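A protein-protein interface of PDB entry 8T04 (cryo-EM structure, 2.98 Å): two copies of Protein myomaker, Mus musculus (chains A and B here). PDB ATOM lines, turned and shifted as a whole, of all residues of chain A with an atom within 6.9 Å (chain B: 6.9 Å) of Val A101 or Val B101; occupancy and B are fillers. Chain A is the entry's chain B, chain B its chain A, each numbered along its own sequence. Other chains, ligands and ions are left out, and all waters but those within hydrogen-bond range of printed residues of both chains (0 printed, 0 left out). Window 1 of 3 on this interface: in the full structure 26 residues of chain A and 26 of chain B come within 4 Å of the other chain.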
ATOM      1  N   VAL A  36     -19.130   0.198  25.325  1.00  0.00           N
ATOM      2  CA  VAL A  36     -20.230   0.877  24.573  1.00  0.00           C
ATOM      3  C   VAL A  36     -20.100   2.394  24.764  1.00  0.00           C
ATOM      4  O   VAL A  36     -20.306   3.118  23.773  1.00  0.00           O
ATOM      5  CB  VAL A  36     -21.621   0.352  24.985  1.00  0.00           C
ATOM      6  CG1 VAL A  36     -22.755   1.139  24.344  1.00  0.00           C
ATOM      7  CG2 VAL A  36     -21.781  -1.125  24.662  1.00  0.00           C
ATOM      8  N   PHE A  39     -16.716   3.474  22.868  1.00  0.00           N
ATOM      9  CA  PHE A  39     -17.118   3.381  21.437  1.00  0.00           C
ATOM     10  C   PHE A  39     -17.943   4.621  21.071  1.00  0.00           C
ATOM     11  O   PHE A  39     -17.614   5.281  20.067  1.00  0.00           O
ATOM     12  CB  PHE A  39     -17.890   2.079  21.202  1.00  0.00           C
ATOM     13  CG  PHE A  39     -18.342   1.823  19.786  1.00  0.00           C
ATOM     14  CD1 PHE A  39     -19.600   2.224  19.357  1.00  0.00           C
ATOM     15  CD2 PHE A  39     -17.525   1.146  18.892  1.00  0.00           C
ATOM     16  CE1 PHE A  39     -20.021   1.972  18.059  1.00  0.00           C
ATOM     17  CE2 PHE A  39     -17.949   0.891  17.595  1.00  0.00           C
ATOM     18  CZ  PHE A  39     -19.194   1.308  17.179  1.00  0.00           C
ATOM     19  N   PHE A  69     -22.415   5.623  13.593  1.00  0.00           N
ATOM     20  CA  PHE A  69     -21.902   5.007  14.850  1.00  0.00           C
ATOM     21  C   PHE A  69     -21.916   6.017  16.004  1.00  0.00           C
ATOM     22  O   PHE A  69     -21.790   5.579  17.165  1.00  0.00           O
ATOM     23  CB  PHE A  69     -20.524   4.381  14.626  1.00  0.00           C
ATOM     24  CG  PHE A  69     -20.613   3.112  13.821  1.00  0.00           C
ATOM     25  CD1 PHE A  69     -21.302   2.018  14.322  1.00  0.00           C
ATOM     26  CD2 PHE A  69     -20.075   3.028  12.545  1.00  0.00           C
ATOM     27  CE1 PHE A  69     -21.422   0.854  13.581  1.00  0.00           C
ATOM     28  CE2 PHE A  69     -20.196   1.862  11.804  1.00  0.00           C
ATOM     29  CZ  PHE A  69     -20.873   0.780  12.322  1.00  0.00           C
ATOM     30  N   TYR A  72     -25.893   5.251  16.589  1.00  0.00           N
ATOM     31  CA  TYR A  72     -26.012   3.825  17.006  1.00  0.00           C
ATOM     32  C   TYR A  72     -25.406   3.640  18.404  1.00  0.00           C
ATOM     33  O   TYR A  72     -26.073   3.022  19.259  1.00  0.00           O
ATOM     34  CB  TYR A  72     -25.353   2.894  15.985  1.00  0.00           C
ATOM     35  CG  TYR A  72     -25.224   1.462  16.442  1.00  0.00           C
ATOM     36  CD1 TYR A  72     -26.326   0.622  16.482  1.00  0.00           C
ATOM     37  CD2 TYR A  72     -24.002   0.949  16.852  1.00  0.00           C
ATOM     38  CE1 TYR A  72     -26.218  -0.693  16.909  1.00  0.00           C
ATOM     39  CE2 TYR A  72     -23.876  -0.363  17.282  1.00  0.00           C
ATOM     40  CZ  TYR A  72     -24.988  -1.188  17.309  1.00  0.00           C
ATOM     41  OH  TYR A  72     -24.875  -2.482  17.729  1.00  0.00           O
ATOM     42  N   LEU A  76     -27.402   2.713  21.795  1.00  0.00           N
ATOM     43  CA  LEU A  76     -26.974   1.449  22.458  1.00  0.00           C
ATOM     44  C   LEU A  76     -26.496   1.742  23.888  1.00  0.00           C
ATOM     45  O   LEU A  76     -26.709   0.868  24.751  1.00  0.00           O
ATOM     46  CB  LEU A  76     -25.886   0.757  21.628  1.00  0.00           C
ATOM     47  CG  LEU A  76     -25.421  -0.610  22.141  1.00  0.00           C
ATOM     48  CD1 LEU A  76     -26.558  -1.624  22.158  1.00  0.00           C
ATOM     49  CD2 LEU A  76     -24.267  -1.138  21.303  1.00  0.00           C
ATOM     50  N   TRP A  79     -29.525   1.821  25.968  1.00  0.00           N
ATOM     51  CA  TRP A  79     -30.004   0.429  26.184  1.00  0.00           C
ATOM     52  C   TRP A  79     -29.198  -0.237  27.309  1.00  0.00           C
ATOM     53  O   TRP A  79     -29.838  -0.705  28.272  1.00  0.00           O
ATOM     54  CB  TRP A  79     -29.971  -0.393  24.887  1.00  0.00           C
ATOM     55  CG  TRP A  79     -30.460  -1.797  25.070  1.00  0.00           C
ATOM     56  CD1 TRP A  79     -29.692  -2.909  25.250  1.00  0.00           C
ATOM     57  CD2 TRP A  79     -31.829  -2.241  25.139  1.00  0.00           C
ATOM     58  NE1 TRP A  79     -30.483  -4.014  25.408  1.00  0.00           N
ATOM     59  CE2 TRP A  79     -31.799  -3.638  25.346  1.00  0.00           C
ATOM     60  CE3 TRP A  79     -33.073  -1.603  25.039  1.00  0.00           C
ATOM     61  CZ2 TRP A  79     -32.963  -4.402  25.449  1.00  0.00           C
ATOM     62  CZ3 TRP A  79     -34.222  -2.358  25.143  1.00  0.00           C
ATOM     63  CH2 TRP A  79     -34.164  -3.739  25.350  1.00  0.00           C
ATOM     64  N   VAL A  80     -27.862  -0.278  27.207  1.00  0.00           N
ATOM     65  CA  VAL A  80     -26.995  -1.080  28.130  1.00  0.00           C
ATOM     66  C   VAL A  80     -26.961  -0.444  29.529  1.00  0.00           C
ATOM     67  O   VAL A  80     -26.745  -1.207  30.492  1.00  0.00           O
ATOM     68  CB  VAL A  80     -25.572  -1.333  27.584  1.00  0.00           C
ATOM     69  CG1 VAL A  80     -25.606  -2.093  26.266  1.00  0.00           C
ATOM     70  CG2 VAL A  80     -24.725  -0.073  27.461  1.00  0.00           C
ATOM     71  N   PHE A  96     -31.128 -10.157  26.584  1.00  0.00           N
ATOM     72  CA  PHE A  96     -31.636  -8.759  26.573  1.00  0.00           C
ATOM     73  C   PHE A  96     -30.561  -7.825  26.005  1.00  0.00           C
ATOM     74  O   PHE A  96     -30.949  -6.936  25.232  1.00  0.00           O
ATOM     75  CB  PHE A  96     -32.155  -8.324  27.948  1.00  0.00           C
ATOM     76  CG  PHE A  96     -33.557  -8.796  28.246  1.00  0.00           C
ATOM     77  CD1 PHE A  96     -34.620  -8.404  27.445  1.00  0.00           C
ATOM     78  CD2 PHE A  96     -33.817  -9.639  29.318  1.00  0.00           C
ATOM     79  CE1 PHE A  96     -35.909  -8.846  27.706  1.00  0.00           C
ATOM     80  CE2 PHE A  96     -35.108 -10.078  29.580  1.00  0.00           C
ATOM     81  CZ  PHE A  96     -36.151  -9.680  28.775  1.00  0.00           C
ATOM     82  N   THR A  97     -29.276  -8.036  26.327  1.00  0.00           N
ATOM     83  CA  THR A  97     -28.143  -7.275  25.725  1.00  0.00           C
ATOM     84  C   THR A  97     -28.182  -7.419  24.198  1.00  0.00           C
ATOM     85  O   THR A  97     -28.094  -6.381  23.514  1.00  0.00           O
ATOM     86  CB  THR A  97     -26.773  -7.703  26.265  1.00  0.00           C
ATOM     87  OG1 THR A  97     -26.796  -7.588  27.687  1.00  0.00           O
ATOM     88  CG2 THR A  97     -25.643  -6.865  25.699  1.00  0.00           C
ATOM     89  N   MET A  98     -28.313  -8.650  23.695  1.00  0.00           N
ATOM     90  CA  MET A  98     -28.289  -8.965  22.240  1.00  0.00           C
ATOM     91  C   MET A  98     -29.551  -8.417  21.560  1.00  0.00           C
ATOM     92  O   MET A  98     -29.431  -7.951  20.410  1.00  0.00           O
ATOM     93  CB  MET A  98     -28.183 -10.475  22.000  1.00  0.00           C
ATOM     94  CG  MET A  98     -27.832 -10.854  20.568  1.00  0.00           C
ATOM     95  SD  MET A  98     -26.043 -10.926  20.272  1.00  0.00           S
ATOM     96  CE  MET A  98     -25.659  -9.205  19.951  1.00  0.00           C
ATOM     97  N   LEU A  99     -30.704  -8.465  22.236  1.00  0.00           N
ATOM     98  CA  LEU A  99     -32.002  -7.949  21.718  1.00  0.00           C
ATOM     99  C   LEU A  99     -31.864  -6.463  21.359  1.00  0.00           C
ATOM    100  O   LEU A  99     -32.315  -6.088  20.261  1.00  0.00           O
ATOM    101  CB  LEU A  99     -33.095  -8.181  22.767  1.00  0.00           C
ATOM    102  CG  LEU A  99     -34.477  -7.629  22.425  1.00  0.00           C
ATOM    103  CD1 LEU A  99     -35.089  -8.332  21.223  1.00  0.00           C
ATOM    104  CD2 LEU A  99     -35.402  -7.719  23.629  1.00  0.00           C
ATOM    105  N   GLY A 100     -31.264  -5.658  22.245  1.00  0.00           N
ATOM    106  CA  GLY A 100     -30.995  -4.225  22.013  1.00  0.00           C
ATOM    107  C   GLY A 100     -30.053  -4.018  20.840  1.00  0.00           C
ATOM    108  O   GLY A 100     -30.414  -3.252  19.934  1.00  0.00           O
ATOM    109  N   VAL A 101     -28.904  -4.703  20.853  1.00  0.00           N
ATOM    110  CA  VAL A 101     -27.855  -4.646  19.788  1.00  0.00           C
ATOM    111  C   VAL A 101     -28.516  -4.844  18.419  1.00  0.00           C
ATOM    112  O   VAL A 101     -28.368  -3.948  17.566  1.00  0.00           O
ATOM    113  CB  VAL A 101     -26.742  -5.687  20.031  1.00  0.00           C
ATOM    114  CG1 VAL A 101     -25.895  -5.949  18.791  1.00  0.00           C
ATOM    115  CG2 VAL A 101     -25.853  -5.282  21.194  1.00  0.00           C
ATOM    116  N   LEU A 102     -29.215  -5.967  18.229  1.00  0.00           N
ATOM    117  CA  LEU A 102     -29.725  -6.411  16.903  1.00  0.00           C
ATOM    118  C   LEU A 102     -30.875  -5.507  16.437  1.00  0.00           C
ATOM    119  O   LEU A 102     -30.876  -5.165  15.241  1.00  0.00           O
ATOM    120  CB  LEU A 102     -30.151  -7.884  16.969  1.00  0.00           C
ATOM    121  CG  LEU A 102     -29.034  -8.891  17.253  1.00  0.00           C
ATOM    122  CD1 LEU A 102     -29.603 -10.295  17.404  1.00  0.00           C
ATOM    123  CD2 LEU A 102     -27.965  -8.877  16.167  1.00  0.00           C
ATOM    124  N   THR A 103     -31.800  -5.117  17.322  1.00  0.00           N
ATOM    125  CA  THR A 103     -32.978  -4.275  16.956  1.00  0.00           C
ATOM    126  C   THR A 103     -32.558  -2.815  16.727  1.00  0.00           C
ATOM    127  O   THR A 103     -33.123  -2.198  15.801  1.00  0.00           O
ATOM    128  CB  THR A 103     -34.106  -4.373  17.989  1.00  0.00           C
ATOM    129  OG1 THR A 103     -33.562  -3.974  19.247  1.00  0.00           O
ATOM    130  CG2 THR A 103     -34.708  -5.758  18.073  1.00  0.00           C
ATOM    131  N   ILE A 104     -31.629  -2.275  17.528  1.00  0.00           N
ATOM    132  CA  ILE A 104     -31.121  -0.873  17.385  1.00  0.00           C
ATOM    133  C   ILE A 104     -30.266  -0.781  16.112  1.00  0.00           C
ATOM    134  O   ILE A 104     -30.356   0.261  15.433  1.00  0.00           O
ATOM    135  CB  ILE A 104     -30.370  -0.396  18.650  1.00  0.00           C
ATOM    136  CG1 ILE A 104     -31.312  -0.329  19.856  1.00  0.00           C
ATOM    137  CG2 ILE A 104     -29.678   0.944  18.421  1.00  0.00           C
ATOM    138  CD1 ILE A 104     -30.617  -0.192  21.194  1.00  0.00           C
ATOM    139  N   ALA A 105     -29.481  -1.820  15.798  1.00  0.00           N
ATOM    140  CA  ALA A 105     -28.640  -1.905  14.579  1.00  0.00           C
ATOM    141  C   ALA A 105     -29.524  -1.760  13.335  1.00  0.00           C
ATOM    142  O   ALA A 105     -29.233  -0.866  12.516  1.00  0.00           O
ATOM    143  CB  ALA A 105     -27.863  -3.199  14.550  1.00  0.00           C
ATOM    144  N   VAL A 106     -30.575  -2.584  13.221  1.00  0.00           N
ATOM    145  CA  VAL A 106     -31.514  -2.599  12.057  1.00  0.00           C
ATOM    146  C   VAL A 106     -32.281  -1.277  12.019  1.00  0.00           C
ATOM    147  O   VAL A 106     -32.425  -0.723  10.908  1.00  0.00           O
ATOM    148  CB  VAL A 106     -32.484  -3.797  12.084  1.00  0.00           C
ATOM    149  CG1 VAL A 106     -33.519  -3.722  10.965  1.00  0.00           C
ATOM    150  CG2 VAL A 106     -31.743  -5.121  12.010  1.00  0.00           C
ATOM    151  N   VAL B  36     -28.871 -14.691  17.358  1.00  0.00           N
ATOM    152  CA  VAL B  36     -27.910 -14.301  16.280  1.00  0.00           C
ATOM    153  C   VAL B  36     -28.117 -15.224  15.071  1.00  0.00           C
ATOM    154  O   VAL B  36     -28.079 -14.707  13.940  1.00  0.00           O
ATOM    155  CB  VAL B  36     -26.449 -14.312  16.779  1.00  0.00           C
ATOM    156  CG1 VAL B  36     -25.448 -14.070  15.658  1.00  0.00           C
ATOM    157  CG2 VAL B  36     -26.228 -13.294  17.885  1.00  0.00           C
ATOM    158  N   PHE B  39     -31.752 -14.328  13.597  1.00  0.00           N
ATOM    159  CA  PHE B  39     -31.509 -13.015  12.941  1.00  0.00           C
ATOM    160  C   PHE B  39     -30.809 -13.249  11.597  1.00  0.00           C
ATOM    161  O   PHE B  39     -31.280 -12.710  10.578  1.00  0.00           O
ATOM    162  CB  PHE B  39     -30.687 -12.117  13.871  1.00  0.00           C
ATOM    163  CG  PHE B  39     -30.380 -10.733  13.358  1.00  0.00           C
ATOM    164  CD1 PHE B  39     -29.208 -10.477  12.660  1.00  0.00           C
ATOM    165  CD2 PHE B  39     -31.243  -9.676  13.608  1.00  0.00           C
ATOM    166  CE1 PHE B  39     -28.919  -9.198  12.204  1.00  0.00           C
ATOM    167  CE2 PHE B  39     -30.951  -8.398  13.154  1.00  0.00           C
ATOM    168  CZ  PHE B  39     -29.791  -8.162  12.450  1.00  0.00           C
ATOM    169  N   PHE B  69     -27.288  -6.965   6.606  1.00  0.00           N
ATOM    170  CA  PHE B  69     -27.616  -7.787   7.804  1.00  0.00           C
ATOM    171  C   PHE B  69     -27.542  -9.285   7.482  1.00  0.00           C
ATOM    172  O   PHE B  69     -27.519 -10.087   8.437  1.00  0.00           O
ATOM    173  CB  PHE B  69     -28.965  -7.374   8.395  1.00  0.00           C
ATOM    174  CG  PHE B  69     -28.884  -6.043   9.096  1.00  0.00           C
ATOM    175  CD1 PHE B  69     -28.072  -5.895  10.211  1.00  0.00           C
ATOM    176  CD2 PHE B  69     -29.555  -4.931   8.614  1.00  0.00           C
ATOM    177  CE1 PHE B  69     -27.960  -4.670  10.850  1.00  0.00           C
ATOM    178  CE2 PHE B  69     -29.442  -3.706   9.253  1.00  0.00           C
ATOM    179  CZ  PHE B  69     -28.642  -3.577  10.366  1.00  0.00           C
ATOM    180  N   TYR B  72     -23.477  -9.153   7.986  1.00  0.00           N
ATOM    181  CA  TYR B  72     -23.221  -8.808   9.411  1.00  0.00           C
ATOM    182  C   TYR B  72     -23.657  -9.966  10.318  1.00  0.00           C
ATOM    183  O   TYR B  72     -22.868 -10.351  11.205  1.00  0.00           O
ATOM    184  CB  TYR B  72     -23.925  -7.505   9.800  1.00  0.00           C
ATOM    185  CG  TYR B  72     -23.908  -7.204  11.277  1.00  0.00           C
ATOM    186  CD1 TYR B  72     -22.755  -6.754  11.903  1.00  0.00           C
ATOM    187  CD2 TYR B  72     -25.041  -7.385  12.057  1.00  0.00           C
ATOM    188  CE1 TYR B  72     -22.730  -6.483  13.263  1.00  0.00           C
ATOM    189  CE2 TYR B  72     -25.033  -7.118  13.417  1.00  0.00           C
ATOM    190  CZ  TYR B  72     -23.873  -6.664  14.023  1.00  0.00           C
ATOM    191  OH  TYR B  72     -23.855  -6.399  15.361  1.00  0.00           O
ATOM    192  N   LEU B  76     -21.227 -12.323  12.537  1.00  0.00           N
ATOM    193  CA  LEU B  76     -21.495 -12.307  14.002  1.00  0.00           C
ATOM    194  C   LEU B  76     -21.832 -13.723  14.494  1.00  0.00           C
ATOM    195  O   LEU B  76     -21.473 -14.025  15.647  1.00  0.00           O
ATOM    196  CB  LEU B  76     -22.619 -11.314  14.323  1.00  0.00           C
ATOM    197  CG  LEU B  76     -22.934 -11.116  15.809  1.00  0.00           C
ATOM    198  CD1 LEU B  76     -21.737 -10.558  16.569  1.00  0.00           C
ATOM    199  CD2 LEU B  76     -24.136 -10.204  15.992  1.00  0.00           C
ATOM    200  N   TRP B  79     -18.599 -15.369  15.090  1.00  0.00           N
ATOM    201  CA  TRP B  79     -18.007 -14.842  16.349  1.00  0.00           C
ATOM    202  C   TRP B  79     -18.636 -15.543  17.562  1.00  0.00           C
ATOM    203  O   TRP B  79     -17.863 -16.108  18.360  1.00  0.00           O
ATOM    204  CB  TRP B  79     -18.133 -13.314  16.439  1.00  0.00           C
ATOM    205  CG  TRP B  79     -17.532 -12.750  17.691  1.00  0.00           C
ATOM    206  CD1 TRP B  79     -18.200 -12.410  18.831  1.00  0.00           C
ATOM    207  CD2 TRP B  79     -16.139 -12.498  17.953  1.00  0.00           C
ATOM    208  NE1 TRP B  79     -17.325 -11.949  19.775  1.00  0.00           N
ATOM    209  CE2 TRP B  79     -16.053 -11.991  19.269  1.00  0.00           C
ATOM    210  CE3 TRP B  79     -14.960 -12.642  17.209  1.00  0.00           C
ATOM    211  CZ2 TRP B  79     -14.836 -11.627  19.849  1.00  0.00           C
ATOM    212  CZ3 TRP B  79     -13.758 -12.282  17.784  1.00  0.00           C
ATOM    213  CH2 TRP B  79     -13.701 -11.786  19.088  1.00  0.00           C
ATOM    214  N   VAL B  80     -19.970 -15.519  17.700  1.00  0.00           N
ATOM    215  CA  VAL B  80     -20.674 -15.984  18.939  1.00  0.00           C
ATOM    216  C   VAL B  80     -20.596 -17.514  19.064  1.00  0.00           C
ATOM    217  O   VAL B  80     -20.664 -17.990  20.216  1.00  0.00           O
ATOM    218  CB  VAL B  80     -22.129 -15.478  19.054  1.00  0.00           C
ATOM    219  CG1 VAL B  80     -22.193 -13.958  19.071  1.00  0.00           C
ATOM    220  CG2 VAL B  80     -23.066 -16.047  17.997  1.00  0.00           C
ATOM    221  N   PHE B  96     -16.145  -9.900  25.601  1.00  0.00           N
ATOM    222  CA  PHE B  96     -15.736 -10.546  24.325  1.00  0.00           C
ATOM    223  C   PHE B  96     -16.929 -10.582  23.362  1.00  0.00           C
ATOM    224  O   PHE B  96     -16.690 -10.322  22.172  1.00  0.00           O
ATOM    225  CB  PHE B  96     -15.097 -11.920  24.554  1.00  0.00           C
ATOM    226  CG  PHE B  96     -13.642 -11.855  24.950  1.00  0.00           C
ATOM    227  CD1 PHE B  96     -12.703 -11.281  24.103  1.00  0.00           C
ATOM    228  CD2 PHE B  96     -13.207 -12.355  26.169  1.00  0.00           C
ATOM    229  CE1 PHE B  96     -11.366 -11.207  24.468  1.00  0.00           C
ATOM    230  CE2 PHE B  96     -11.869 -12.284  26.532  1.00  0.00           C
ATOM    231  CZ  PHE B  96     -10.951 -11.710  25.680  1.00  0.00           C
ATOM    232  N   THR B  97     -18.151 -10.843  23.846  1.00  0.00           N
ATOM    233  CA  THR B  97     -19.392 -10.769  23.021  1.00  0.00           C
ATOM    234  C   THR B  97     -19.515  -9.371  22.404  1.00  0.00           C
ATOM    235  O   THR B  97     -19.748  -9.293  21.183  1.00  0.00           O
ATOM    236  CB  THR B  97     -20.663 -11.119  23.808  1.00  0.00           C
ATOM    237  OG1 THR B  97     -20.486 -12.412  24.388  1.00  0.00           O
ATOM    238  CG2 THR B  97     -21.902 -11.113  22.935  1.00  0.00           C
ATOM    239  N   MET B  98     -19.357  -8.318  23.214  1.00  0.00           N
ATOM    240  CA  MET B  98     -19.524  -6.902  22.787  1.00  0.00           C
ATOM    241  C   MET B  98     -18.385  -6.496  21.843  1.00  0.00           C
ATOM    242  O   MET B  98     -18.660  -5.727  20.903  1.00  0.00           O
ATOM    243  CB  MET B  98     -19.560  -5.959  23.995  1.00  0.00           C
ATOM    244  CG  MET B  98     -20.047  -4.553  23.671  1.00  0.00           C
ATOM    245  SD  MET B  98     -21.848  -4.379  23.796  1.00  0.00           S
ATOM    246  CE  MET B  98     -22.379  -4.968  22.190  1.00  0.00           C
ATOM    247  N   LEU B  99     -17.164  -6.992  22.076  1.00  0.00           N
ATOM    248  CA  LEU B  99     -15.970  -6.710  21.231  1.00  0.00           C
ATOM    249  C   LEU B  99     -16.245  -7.139  19.783  1.00  0.00           C
ATOM    250  O   LEU B  99     -15.940  -6.345  18.875  1.00  0.00           O
ATOM    251  CB  LEU B  99     -14.753  -7.433  21.818  1.00  0.00           C
ATOM    252  CG  LEU B  99     -13.458  -7.317  21.017  1.00  0.00           C
ATOM    253  CD1 LEU B  99     -12.939  -5.887  20.979  1.00  0.00           C
ATOM    254  CD2 LEU B  99     -12.399  -8.258  21.575  1.00  0.00           C
ATOM    255  N   GLY B 100     -16.798  -8.341  19.581  1.00  0.00           N
ATOM    256  CA  GLY B 100     -17.184  -8.863  18.256  1.00  0.00           C
ATOM    257  C   GLY B 100     -18.265  -8.011  17.615  1.00  0.00           C
ATOM    258  O   GLY B 100     -18.062  -7.582  16.469  1.00  0.00           O
ATOM    259  N   VAL B 101     -19.356  -7.758  18.345  1.00  0.00           N
ATOM    260  CA  VAL B 101     -20.519  -6.930  17.900  1.00  0.00           C
ATOM    261  C   VAL B 101     -20.003  -5.603  17.334  1.00  0.00           C
ATOM    262  O   VAL B 101     -20.299  -5.315  16.160  1.00  0.00           O
ATOM    263  CB  VAL B 101     -21.526  -6.701  19.047  1.00  0.00           C
ATOM    264  CG1 VAL B 101     -22.486  -5.550  18.770  1.00  0.00           C
ATOM    265  CG2 VAL B 101     -22.304  -7.968  19.358  1.00  0.00           C
ATOM    266  N   LEU B 102     -19.259  -4.837  18.140  1.00  0.00           N
ATOM    267  CA  LEU B 102     -18.872  -3.434  17.825  1.00  0.00           C
ATOM    268  C   LEU B 102     -17.846  -3.401  16.685  1.00  0.00           C
ATOM    269  O   LEU B 102     -18.001  -2.532  15.808  1.00  0.00           O
ATOM    270  CB  LEU B 102     -18.345  -2.738  19.086  1.00  0.00           C
ATOM    271  CG  LEU B 102     -19.354  -2.559  20.224  1.00  0.00           C
ATOM    272  CD1 LEU B 102     -18.679  -1.962  21.449  1.00  0.00           C
ATOM    273  CD2 LEU B 102     -20.536  -1.693  19.807  1.00  0.00           C
ATOM    274  N   THR B 103     -16.852  -4.300  16.670  1.00  0.00           N
ATOM    275  CA  THR B 103     -15.783  -4.320  15.630  1.00  0.00           C
ATOM    276  C   THR B 103     -16.326  -4.862  14.299  1.00  0.00           C
ATOM    277  O   THR B 103     -15.920  -4.316  13.253  1.00  0.00           O
ATOM    278  CB  THR B 103     -14.543  -5.095  16.086  1.00  0.00           C
ATOM    279  OG1 THR B 103     -14.964  -6.420  16.412  1.00  0.00           O
ATOM    280  CG2 THR B 103     -13.844  -4.446  17.261  1.00  0.00           C
ATOM    281  N   ILE B 104     -17.188  -5.887  14.321  1.00  0.00           N
ATOM    282  CA  ILE B 104     -17.801  -6.488  13.093  1.00  0.00           C
ATOM    283  C   ILE B 104     -18.798  -5.484  12.494  1.00  0.00           C
ATOM    284  O   ILE B 104     -18.855  -5.403  11.252  1.00  0.00           O
ATOM    285  CB  ILE B 104     -18.435  -7.869  13.376  1.00  0.00           C
ATOM    286  CG1 ILE B 104     -17.369  -8.887  13.795  1.00  0.00           C
ATOM    287  CG2 ILE B 104     -19.236  -8.375  12.179  1.00  0.00           C
ATOM    288  CD1 ILE B 104     -17.917 -10.161  14.401  1.00  0.00           C
ATOM    289  N   ALA B 105     -19.542  -4.751  13.333  1.00  0.00           N
ATOM    290  CA  ALA B 105     -20.508  -3.707  12.913  1.00  0.00           C
ATOM    291  C   ALA B 105     -19.785  -2.636  12.088  1.00  0.00           C
ATOM    292  O   ALA B 105     -20.231  -2.375  10.955  1.00  0.00           O
ATOM    293  CB  ALA B 105     -21.199  -3.099  14.109  1.00  0.00           C
ATOM    294  N   VAL B 106     -18.698  -2.068  12.626  1.00  0.00           N
ATOM    295  CA  VAL B 106     -17.897  -0.988  11.969  1.00  0.00           C
ATOM    296  C   VAL B 106     -17.229  -1.558  10.717  1.00  0.00           C
ATOM    297  O   VAL B 106     -17.250  -0.858   9.684  1.00  0.00           O
ATOM    298  CB  VAL B 106     -16.852  -0.357  12.912  1.00  0.00           C
ATOM    299  CG1 VAL B 106     -15.958   0.644  12.188  1.00  0.00           C
ATOM    300  CG2 VAL B 106     -17.508   0.310  14.108  1.00  0.00           C
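Among the printed residues, pairs that only touch across the chains: Val A36 with Met B98, Phe A39 with Leu B102, Phe A39 with Val B106, Phe A69 with Ala B105, Phe A69 with Val B106, Met A98 with Val B36, Met A98 with Val B101, Val A101 with Met B98, Val A101 with Val B101, Leu A102 with Phe B39, Ala A105 with Phe B69, Val A106 with Phe B39 and Val A106 with Phe B69.
Of the printed residues of chain B, Val A101 touches Met B98 (3.6 Å) and Val B101 (3.4 Å).
Of the printed residues of chain B, Ala A105 touches Phe B69 (3.5 Å).
Of the printed residues of chain A, Phe B39 touches Leu A102 and Val A106.
Of chain A, only Met A98 and Val A101 come within 4 Å of Val B101.
The nearest printed residue of chain B that does not touch Val A101 is Tyr B72 (4.02 Å).
The nearest printed residue of chain A that does not touch Phe B69 is Leu A102 (5.3 Å).
Of the 18 printed residues of chain A, 8 touch a printed residue of chain B.
Printed residues of chain A that touch a printed residue of chain B: Val A36, Phe A39, Phe A69, Met A98, Val A101, Leu A102, Ala A105 and Val A106.
Hydrophobic or aromatic side chains of chain A that line the printed part of chain B: Val A36, Phe A39, Phe A69, Met A98, Val A101, Leu A102, Ala A105 and Val A106.
Of the 18 printed residues of chain B, 8 touch a printed residue of chain A.
Hydrophobic or aromatic side chains of chain B within 4 Å of the printed part of chain A: Val B36, Phe B39, Phe B69, Met B98, Val B101, Leu B102, Ala B105 and Val B106.
Val A36 touches Met B98, and with the chains exchanged Met A98 touches Val B36.
Phe A69 touches Ala B105, and with the chains exchanged Ala A105 touches Phe B69.
Phe A69 touches Val B106, and with the chains exchanged Val A106 touches Phe B69.
Val A101 touches its own counterpart, Val B101.
Of the 13 pairs that touch across the chains among the printed residues, 13 have their exchanged pair printed and touching as well.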
